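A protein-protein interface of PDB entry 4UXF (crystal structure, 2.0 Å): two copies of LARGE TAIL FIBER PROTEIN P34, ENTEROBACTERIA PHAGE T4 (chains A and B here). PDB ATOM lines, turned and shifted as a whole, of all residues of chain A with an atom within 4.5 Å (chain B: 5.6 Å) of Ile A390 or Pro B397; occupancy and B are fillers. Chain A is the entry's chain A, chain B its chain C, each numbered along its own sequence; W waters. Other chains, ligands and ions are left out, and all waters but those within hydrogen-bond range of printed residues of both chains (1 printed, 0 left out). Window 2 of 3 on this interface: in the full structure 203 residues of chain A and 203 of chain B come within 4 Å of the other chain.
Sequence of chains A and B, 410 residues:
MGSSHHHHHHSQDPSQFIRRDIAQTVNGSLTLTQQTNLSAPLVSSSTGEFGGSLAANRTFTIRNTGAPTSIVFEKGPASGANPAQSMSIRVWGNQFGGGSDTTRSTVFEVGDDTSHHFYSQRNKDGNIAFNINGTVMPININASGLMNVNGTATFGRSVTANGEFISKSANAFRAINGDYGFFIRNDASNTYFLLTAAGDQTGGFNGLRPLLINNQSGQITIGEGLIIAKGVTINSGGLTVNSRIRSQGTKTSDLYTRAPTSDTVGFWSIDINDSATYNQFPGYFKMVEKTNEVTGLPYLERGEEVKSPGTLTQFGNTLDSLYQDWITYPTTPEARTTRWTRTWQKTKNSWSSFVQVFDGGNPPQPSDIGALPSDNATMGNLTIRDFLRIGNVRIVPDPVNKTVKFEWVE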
ATOM      1  N   LEU A 388      20.735   8.581  -4.209  1.00  0.00           N
ATOM      2  CA  LEU A 388      19.341   8.837  -3.893  1.00  0.00           C
ATOM      3  C   LEU A 388      19.290   9.378  -2.458  1.00  0.00           C
ATOM      4  O   LEU A 388      19.786   8.741  -1.535  1.00  0.00           O
ATOM      5  CB  LEU A 388      18.517   7.579  -3.990  1.00  0.00           C
ATOM      6  CG  LEU A 388      17.072   7.643  -3.474  1.00  0.00           C
ATOM      7  CD1 LEU A 388      16.215   8.442  -4.424  1.00  0.00           C
ATOM      8  CD2 LEU A 388      16.505   6.247  -3.311  1.00  0.00           C
ATOM      9  N   ARG A 389      18.669  10.527  -2.279  1.00  0.00           N
ATOM     10  CA  ARG A 389      18.414  11.064  -0.974  1.00  0.00           C
ATOM     11  C   ARG A 389      16.918  10.973  -0.659  1.00  0.00           C
ATOM     12  O   ARG A 389      16.076  11.329  -1.504  1.00  0.00           O
ATOM     13  CB  ARG A 389      18.942  12.488  -0.945  1.00  0.00           C
ATOM     14  CG  ARG A 389      18.768  13.132   0.393  1.00  0.00           C
ATOM     15  CD  ARG A 389      19.401  14.500   0.405  1.00  0.00           C
ATOM     16  NE  ARG A 389      19.127  15.136   1.685  1.00  0.00           N
ATOM     17  CZ  ARG A 389      19.430  16.388   1.985  1.00  0.00           C
ATOM     18  NH1 ARG A 389      20.025  17.179   1.095  1.00  0.00           N
ATOM     19  NH2 ARG A 389      19.134  16.855   3.191  1.00  0.00           N
ATOM     20  N   ILE A 390      16.585  10.452   0.525  1.00  0.00           N
ATOM     21  CA  ILE A 390      15.216  10.484   1.056  1.00  0.00           C
ATOM     22  C   ILE A 390      15.262  11.266   2.366  1.00  0.00           C
ATOM     23  O   ILE A 390      15.905  10.824   3.346  1.00  0.00           O
ATOM     24  CB  ILE A 390      14.615   9.091   1.292  1.00  0.00           C
ATOM     25  CG1 ILE A 390      14.689   8.238   0.011  1.00  0.00           C
ATOM     26  CG2 ILE A 390      13.174   9.207   1.766  1.00  0.00           C
ATOM     27  CD1 ILE A 390      14.279   6.804   0.179  1.00  0.00           C
ATOM     28  N   GLY A 391      14.588  12.422   2.380  1.00  0.00           N
ATOM     29  CA  GLY A 391      14.617  13.338   3.512  1.00  0.00           C
ATOM     30  C   GLY A 391      16.065  13.708   3.742  1.00  0.00           C
ATOM     31  O   GLY A 391      16.729  14.237   2.843  1.00  0.00           O
ATOM     32  N   ASN A 392      16.572  13.372   4.922  1.00  0.00           N
ATOM     33  CA  ASN A 392      17.952  13.681   5.293  1.00  0.00           C
ATOM     34  C   ASN A 392      18.932  12.526   5.119  1.00  0.00           C
ATOM     35  O   ASN A 392      20.091  12.680   5.493  1.00  0.00           O
ATOM     36  CB  ASN A 392      18.019  14.150   6.754  1.00  0.00           C
ATOM     37  CG  ASN A 392      17.489  15.547   6.937  1.00  0.00           C
ATOM     38  OD1 ASN A 392      18.159  16.529   6.611  1.00  0.00           O
ATOM     39  ND2 ASN A 392      16.276  15.645   7.449  1.00  0.00           N
ATOM     40  N   VAL A 393      18.507  11.389   4.577  1.00  0.00           N
ATOM     41  CA  VAL A 393      19.454  10.266   4.395  1.00  0.00           C
ATOM     42  C   VAL A 393      19.834  10.095   2.899  1.00  0.00           C
ATOM     43  O   VAL A 393      18.964   9.952   2.061  1.00  0.00           O
ATOM     44  CB  VAL A 393      19.020   8.971   5.154  1.00  0.00           C
ATOM     45  CG1 VAL A 393      17.546   8.647   5.018  1.00  0.00           C
ATOM     46  CG2 VAL A 393      19.872   7.776   4.756  1.00  0.00           C
ATOM     47  N   ILE A 395      21.492   7.740   0.181  1.00  0.00           N
ATOM     48  CA  ILE A 395      21.797   6.346  -0.129  1.00  0.00           C
ATOM     49  C   ILE A 395      22.741   6.300  -1.342  1.00  0.00           C
ATOM     50  O   ILE A 395      22.366   6.736  -2.444  1.00  0.00           O
ATOM     51  CB  ILE A 395      20.529   5.577  -0.455  1.00  0.00           C
ATOM     52  CG1 ILE A 395      19.490   5.821   0.635  1.00  0.00           C
ATOM     53  CG2 ILE A 395      20.852   4.099  -0.668  1.00  0.00           C
ATOM     54  CD1 ILE A 395      18.113   5.287   0.311  1.00  0.00           C
ATOM     55  N   THR B 383      16.463  13.500  -5.262  1.00  0.00           N
ATOM     56  CA  THR B 383      16.114  13.780  -3.876  1.00  0.00           C
ATOM     57  C   THR B 383      14.590  13.698  -3.705  1.00  0.00           C
ATOM     58  O   THR B 383      13.822  14.318  -4.449  1.00  0.00           O
ATOM     59  CB  THR B 383      16.649  15.151  -3.450  1.00  0.00           C
ATOM     60  OG1 THR B 383      18.095  15.179  -3.571  1.00  0.00           O
ATOM     61  CG2 THR B 383      16.220  15.463  -1.989  1.00  0.00           C
ATOM     62  N   ILE B 384      14.168  12.943  -2.698  1.00  0.00           N
ATOM     63  CA  ILE B 384      12.781  12.704  -2.414  1.00  0.00           C
ATOM     64  C   ILE B 384      12.531  13.208  -0.998  1.00  0.00           C
ATOM     65  O   ILE B 384      13.162  12.736  -0.047  1.00  0.00           O
ATOM     66  CB  ILE B 384      12.419  11.216  -2.534  1.00  0.00           C
ATOM     67  CG1 ILE B 384      12.588  10.743  -3.987  1.00  0.00           C
ATOM     68  CG2 ILE B 384      10.997  10.993  -2.078  1.00  0.00           C
ATOM     69  CD1 ILE B 384      12.554   9.257  -4.166  1.00  0.00           C
ATOM     70  N   ARG B 385      11.590  14.138  -0.872  1.00  0.00           N
ATOM     71  CA  ARG B 385      11.350  14.861   0.369  1.00  0.00           C
ATOM     72  C   ARG B 385      10.546  14.041   1.351  1.00  0.00           C
ATOM     73  O   ARG B 385      10.908  13.985   2.510  1.00  0.00           O
ATOM     74  CB  ARG B 385      10.681  16.208   0.087  1.00  0.00           C
ATOM     75  CG  ARG B 385      10.711  17.175   1.272  1.00  0.00           C
ATOM     76  CD  ARG B 385       9.852  18.421   1.032  1.00  0.00           C
ATOM     77  NE  ARG B 385       8.451  18.057   0.858  1.00  0.00           N
ATOM     78  CZ  ARG B 385       7.514  18.829   0.308  1.00  0.00           C
ATOM     79  NH1 ARG B 385       7.783  20.061  -0.103  1.00  0.00           N
ATOM     80  NH2 ARG B 385       6.285  18.342   0.160  1.00  0.00           N
ATOM     81  N   ASP B 386       9.518  13.332   0.892  1.00  0.00           N
ATOM     82  CA  ASP B 386       8.523  12.759   1.767  1.00  0.00           C
ATOM     83  C   ASP B 386       8.581  11.254   1.830  1.00  0.00           C
ATOM     84  O   ASP B 386       8.838  10.707   2.895  1.00  0.00           O
ATOM     85  CB  ASP B 386       7.137  13.266   1.369  1.00  0.00           C
ATOM     86  CG  ASP B 386       7.056  14.793   1.423  1.00  0.00           C
ATOM     87  OD1 ASP B 386       7.680  15.369   2.324  1.00  0.00           O
ATOM     88  OD2 ASP B 386       6.471  15.441   0.535  1.00  0.00           O
ATOM     89  N   PHE B 387       8.387  10.565   0.705  1.00  0.00           N
ATOM     90  CA  PHE B 387       8.539   9.121   0.704  1.00  0.00           C
ATOM     91  C   PHE B 387       8.866   8.557  -0.682  1.00  0.00           C
ATOM     92  O   PHE B 387       8.489   9.116  -1.698  1.00  0.00           O
ATOM     93  CB  PHE B 387       7.306   8.423   1.290  1.00  0.00           C
ATOM     94  CG  PHE B 387       6.071   8.561   0.462  1.00  0.00           C
ATOM     95  CD1 PHE B 387       5.772   7.622  -0.524  1.00  0.00           C
ATOM     96  CD2 PHE B 387       5.181   9.621   0.673  1.00  0.00           C
ATOM     97  CE1 PHE B 387       4.631   7.744  -1.303  1.00  0.00           C
ATOM     98  CE2 PHE B 387       4.032   9.734  -0.084  1.00  0.00           C
ATOM     99  CZ  PHE B 387       3.753   8.800  -1.076  1.00  0.00           C
ATOM    100  N   LEU B 388       9.552   7.422  -0.668  1.00  0.00           N
ATOM    101  CA  LEU B 388       9.736   6.593  -1.832  1.00  0.00           C
ATOM    102  C   LEU B 388       8.940   5.340  -1.544  1.00  0.00           C
ATOM    103  O   LEU B 388       9.134   4.694  -0.513  1.00  0.00           O
ATOM    104  CB  LEU B 388      11.219   6.257  -1.995  1.00  0.00           C
ATOM    105  CG  LEU B 388      11.542   5.221  -3.082  1.00  0.00           C
ATOM    106  CD1 LEU B 388      11.198   5.760  -4.467  1.00  0.00           C
ATOM    107  CD2 LEU B 388      13.016   4.835  -2.980  1.00  0.00           C
ATOM    108  N   ILE B 395       9.202   3.951   2.016  1.00  0.00           N
ATOM    109  CA  ILE B 395      10.503   4.143   2.604  1.00  0.00           C
ATOM    110  C   ILE B 395      10.537   5.624   2.961  1.00  0.00           C
ATOM    111  O   ILE B 395      10.400   6.502   2.102  1.00  0.00           O
ATOM    112  CB  ILE B 395      11.640   3.787   1.636  1.00  0.00           C
ATOM    113  CG1 ILE B 395      11.570   2.301   1.256  1.00  0.00           C
ATOM    114  CG2 ILE B 395      12.981   4.157   2.251  1.00  0.00           C
ATOM    115  CD1 ILE B 395      12.406   1.887   0.066  1.00  0.00           C
ATOM    116  N   VAL B 396      10.685   5.897   4.254  1.00  0.00           N
ATOM    117  CA  VAL B 396      10.612   7.255   4.784  1.00  0.00           C
ATOM    118  C   VAL B 396      11.838   7.467   5.654  1.00  0.00           C
ATOM    119  O   VAL B 396      12.522   6.492   6.003  1.00  0.00           O
ATOM    120  CB  VAL B 396       9.321   7.465   5.590  1.00  0.00           C
ATOM    121  CG1 VAL B 396       8.108   7.074   4.756  1.00  0.00           C
ATOM    122  CG2 VAL B 396       9.358   6.651   6.885  1.00  0.00           C
ATOM    123  N   PRO B 397      12.147   8.729   5.973  1.00  0.00           N
ATOM    124  CA  PRO B 397      13.286   8.940   6.866  1.00  0.00           C
ATOM    125  C   PRO B 397      12.907   8.681   8.348  1.00  0.00           C
ATOM    126  O   PRO B 397      11.733   8.879   8.744  1.00  0.00           O
ATOM    127  CB  PRO B 397      13.679  10.399   6.605  1.00  0.00           C
ATOM    128  CG  PRO B 397      12.448  11.054   6.067  1.00  0.00           C
ATOM    129  CD  PRO B 397      11.551   9.994   5.499  1.00  0.00           C
ATOM    130  N   ASP B 398      13.883   8.197   9.124  1.00  0.00           N
ATOM    131  CA  ASP B 398      13.755   8.089  10.588  1.00  0.00           C
ATOM    132  C   ASP B 398      14.925   8.803  11.283  1.00  0.00           C
ATOM    133  O   ASP B 398      16.021   8.217  11.409  1.00  0.00           O
ATOM    134  CB  ASP B 398      13.684   6.622  11.032  1.00  0.00           C
ATOM    135  CG  ASP B 398      13.161   6.465  12.464  1.00  0.00           C
ATOM    136  OD1 ASP B 398      12.318   7.284  12.898  1.00  0.00           O
ATOM    137  OD2 ASP B 398      13.579   5.509  13.152  1.00  0.00           O
ATOM    138  N   PRO B 399      14.714  10.082  11.692  1.00  0.00           N
ATOM    139  CA  PRO B 399      15.722  10.849  12.456  1.00  0.00           C
ATOM    140  C   PRO B 399      16.219  10.146  13.727  1.00  0.00           C
ATOM    141  O   PRO B 399      17.438   9.959  13.892  1.00  0.00           O
ATOM    142  CB  PRO B 399      14.993  12.166  12.769  1.00  0.00           C
ATOM    143  CG  PRO B 399      14.089  12.355  11.599  1.00  0.00           C
ATOM    144  CD  PRO B 399      13.630  10.968  11.209  1.00  0.00           C
ATOM    145  N   THR B 403      18.666   6.972   9.867  1.00  0.00           N
ATOM    146  CA  THR B 403      18.471   6.069   8.717  1.00  0.00           C
ATOM    147  C   THR B 403      17.020   6.132   8.166  1.00  0.00           C
ATOM    148  O   THR B 403      16.264   7.080   8.447  1.00  0.00           O
ATOM    149  CB  THR B 403      18.969   4.614   9.057  1.00  0.00           C
ATOM    150  OG1 THR B 403      19.364   3.925   7.863  1.00  0.00           O
ATOM    151  CG2 THR B 403      17.926   3.776   9.810  1.00  0.00           C
ATOM    152  N   VAL B 404      16.669   5.145   7.347  1.00  0.00           N
ATOM    153  CA  VAL B 404      15.323   5.013   6.776  1.00  0.00           C
ATOM    154  C   VAL B 404      14.521   3.936   7.502  1.00  0.00           C
ATOM    155  O   VAL B 404      15.105   3.000   8.045  1.00  0.00           O
ATOM    156  CB  VAL B 404      15.369   4.646   5.261  1.00  0.00           C
ATOM    157  CG1 VAL B 404      16.157   5.679   4.474  1.00  0.00           C
ATOM    158  CG2 VAL B 404      15.926   3.240   5.008  1.00  0.00           C
ATOM    159  N   LYS B 405      13.192   4.049   7.474  1.00  0.00           N
ATOM    160  CA  LYS B 405      12.326   2.963   7.931  1.00  0.00           C
ATOM    161  C   LYS B 405      11.248   2.610   6.896  1.00  0.00           C
ATOM    162  O   LYS B 405      10.869   3.442   6.064  1.00  0.00           O
ATOM    163  CB  LYS B 405      11.701   3.300   9.281  1.00  0.00           C
ATOM    164  CG  LYS B 405      10.911   4.585   9.313  1.00  0.00           C
ATOM    165  CD  LYS B 405      10.400   4.843  10.717  1.00  0.00           C
ATOM    166  CE  LYS B 405       9.823   6.236  10.883  1.00  0.00           C
ATOM    167  NZ  LYS B 405       8.421   6.295  10.388  1.00  0.00           N
HETATM  168  O   HOH W   1      19.998  16.547  -2.273  1.00  0.00           O
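The backbone NH (N) of Ile B384 is in hydrogen-bond range of the backbone carbonyl oxygen (O) of Arg A389, at 2.8 Å.
The backbone NH (N) of Gly A391 sits at hydrogen-bond distance from the backbone carbonyl oxygen (O) of Ile B384 (2.8 Å).
The guanidinium group (NE) of Arg A389 is in hydrogen-bond range of the backbone carbonyl oxygen (O) of Gly A391 (2.8 Å).
The backbone NH (N) of Asp B398 sits at hydrogen-bond distance from the backbone carbonyl oxygen (O) of Thr B403 (2.7 Å).
OD2 of Asp B386 is in salt-bridge range of NH2 of Arg B385, 2.9 Å away.
O of Leu B388 lies within hydrogen-bond range of N of Ile B395 (2.6 Å).
The backbone carbonyl oxygen (O) of Leu A388 lies within hydrogen-bond range of the backbone NH (N) of Ile A395 (2.6 Å).
Among the printed residues, pairs that only touch across the chains: Ile A390 with Ile B384 (3.2 Å), Val A393 with Val B404 (3.3 Å), Arg A389 with Thr B383 (3.4 Å), Ile A390 with Ile B395 (3.6 Å), Leu A388 with Ile B384 (3.8 Å), Leu A388 with Leu B388 (3.8 Å), Ile A390 with Leu B388 (3.8 Å), Gly A391 with Arg B385 (3.9 Å), Ile A390 with Pro B397 (3.97 Å) and Val A393 with Thr B403 (3.98 Å).
Printed residues of chain B within 4 Å of Arg A389: Thr B383 (3.4 Å) and Ile B384 (2.8 Å).
Printed residues of chain B within 4 Å of Ile A390: Ile B384, Leu B388, Ile B395 and Pro B397.
Ile A395 touches none of the printed residues of chain B.
Of the printed residues of chain A, Ile B384 touches Leu A388, Arg A389, Ile A390 and Gly A391.
Of the printed residues of chain A, Leu B388 touches Leu A388 and Ile A390.
Val B396 touches none of the printed residues of chain A.
The nearest residue of chain A that does not touch Pro B397 is Gly A391 (4.1 Å).
The nearest printed residue of chain B that does not touch Val A393 is Pro B397 (4.5 Å).
Of the 7 printed residues of chain A, 5 touch a printed residue of chain B.
Printed residues of chain A that touch a printed residue of chain B: Leu A388, Arg A389, Ile A390, Gly A391 and Val A393.
Of the 14 printed residues of chain B, 8 touch a printed residue of chain A.
Hydrophobic or aromatic side chains of chain B within 4 Å of the printed part of chain A: Ile B384, Leu B388, Ile B395, Pro B397 and Val B404.
Leu B388 touches its own counterpart, Leu A388.
Of the 12 pairs that touch across the chains among the printed residues, 1 has its exchanged pair printed and touching as well.
Water W1 lies within hydrogen-bond range of the side-chain hydroxyl (OG1) of Thr B383 (2.7 Å) and the guanidinium group (NH1) of Arg A389 (3.4 Å).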
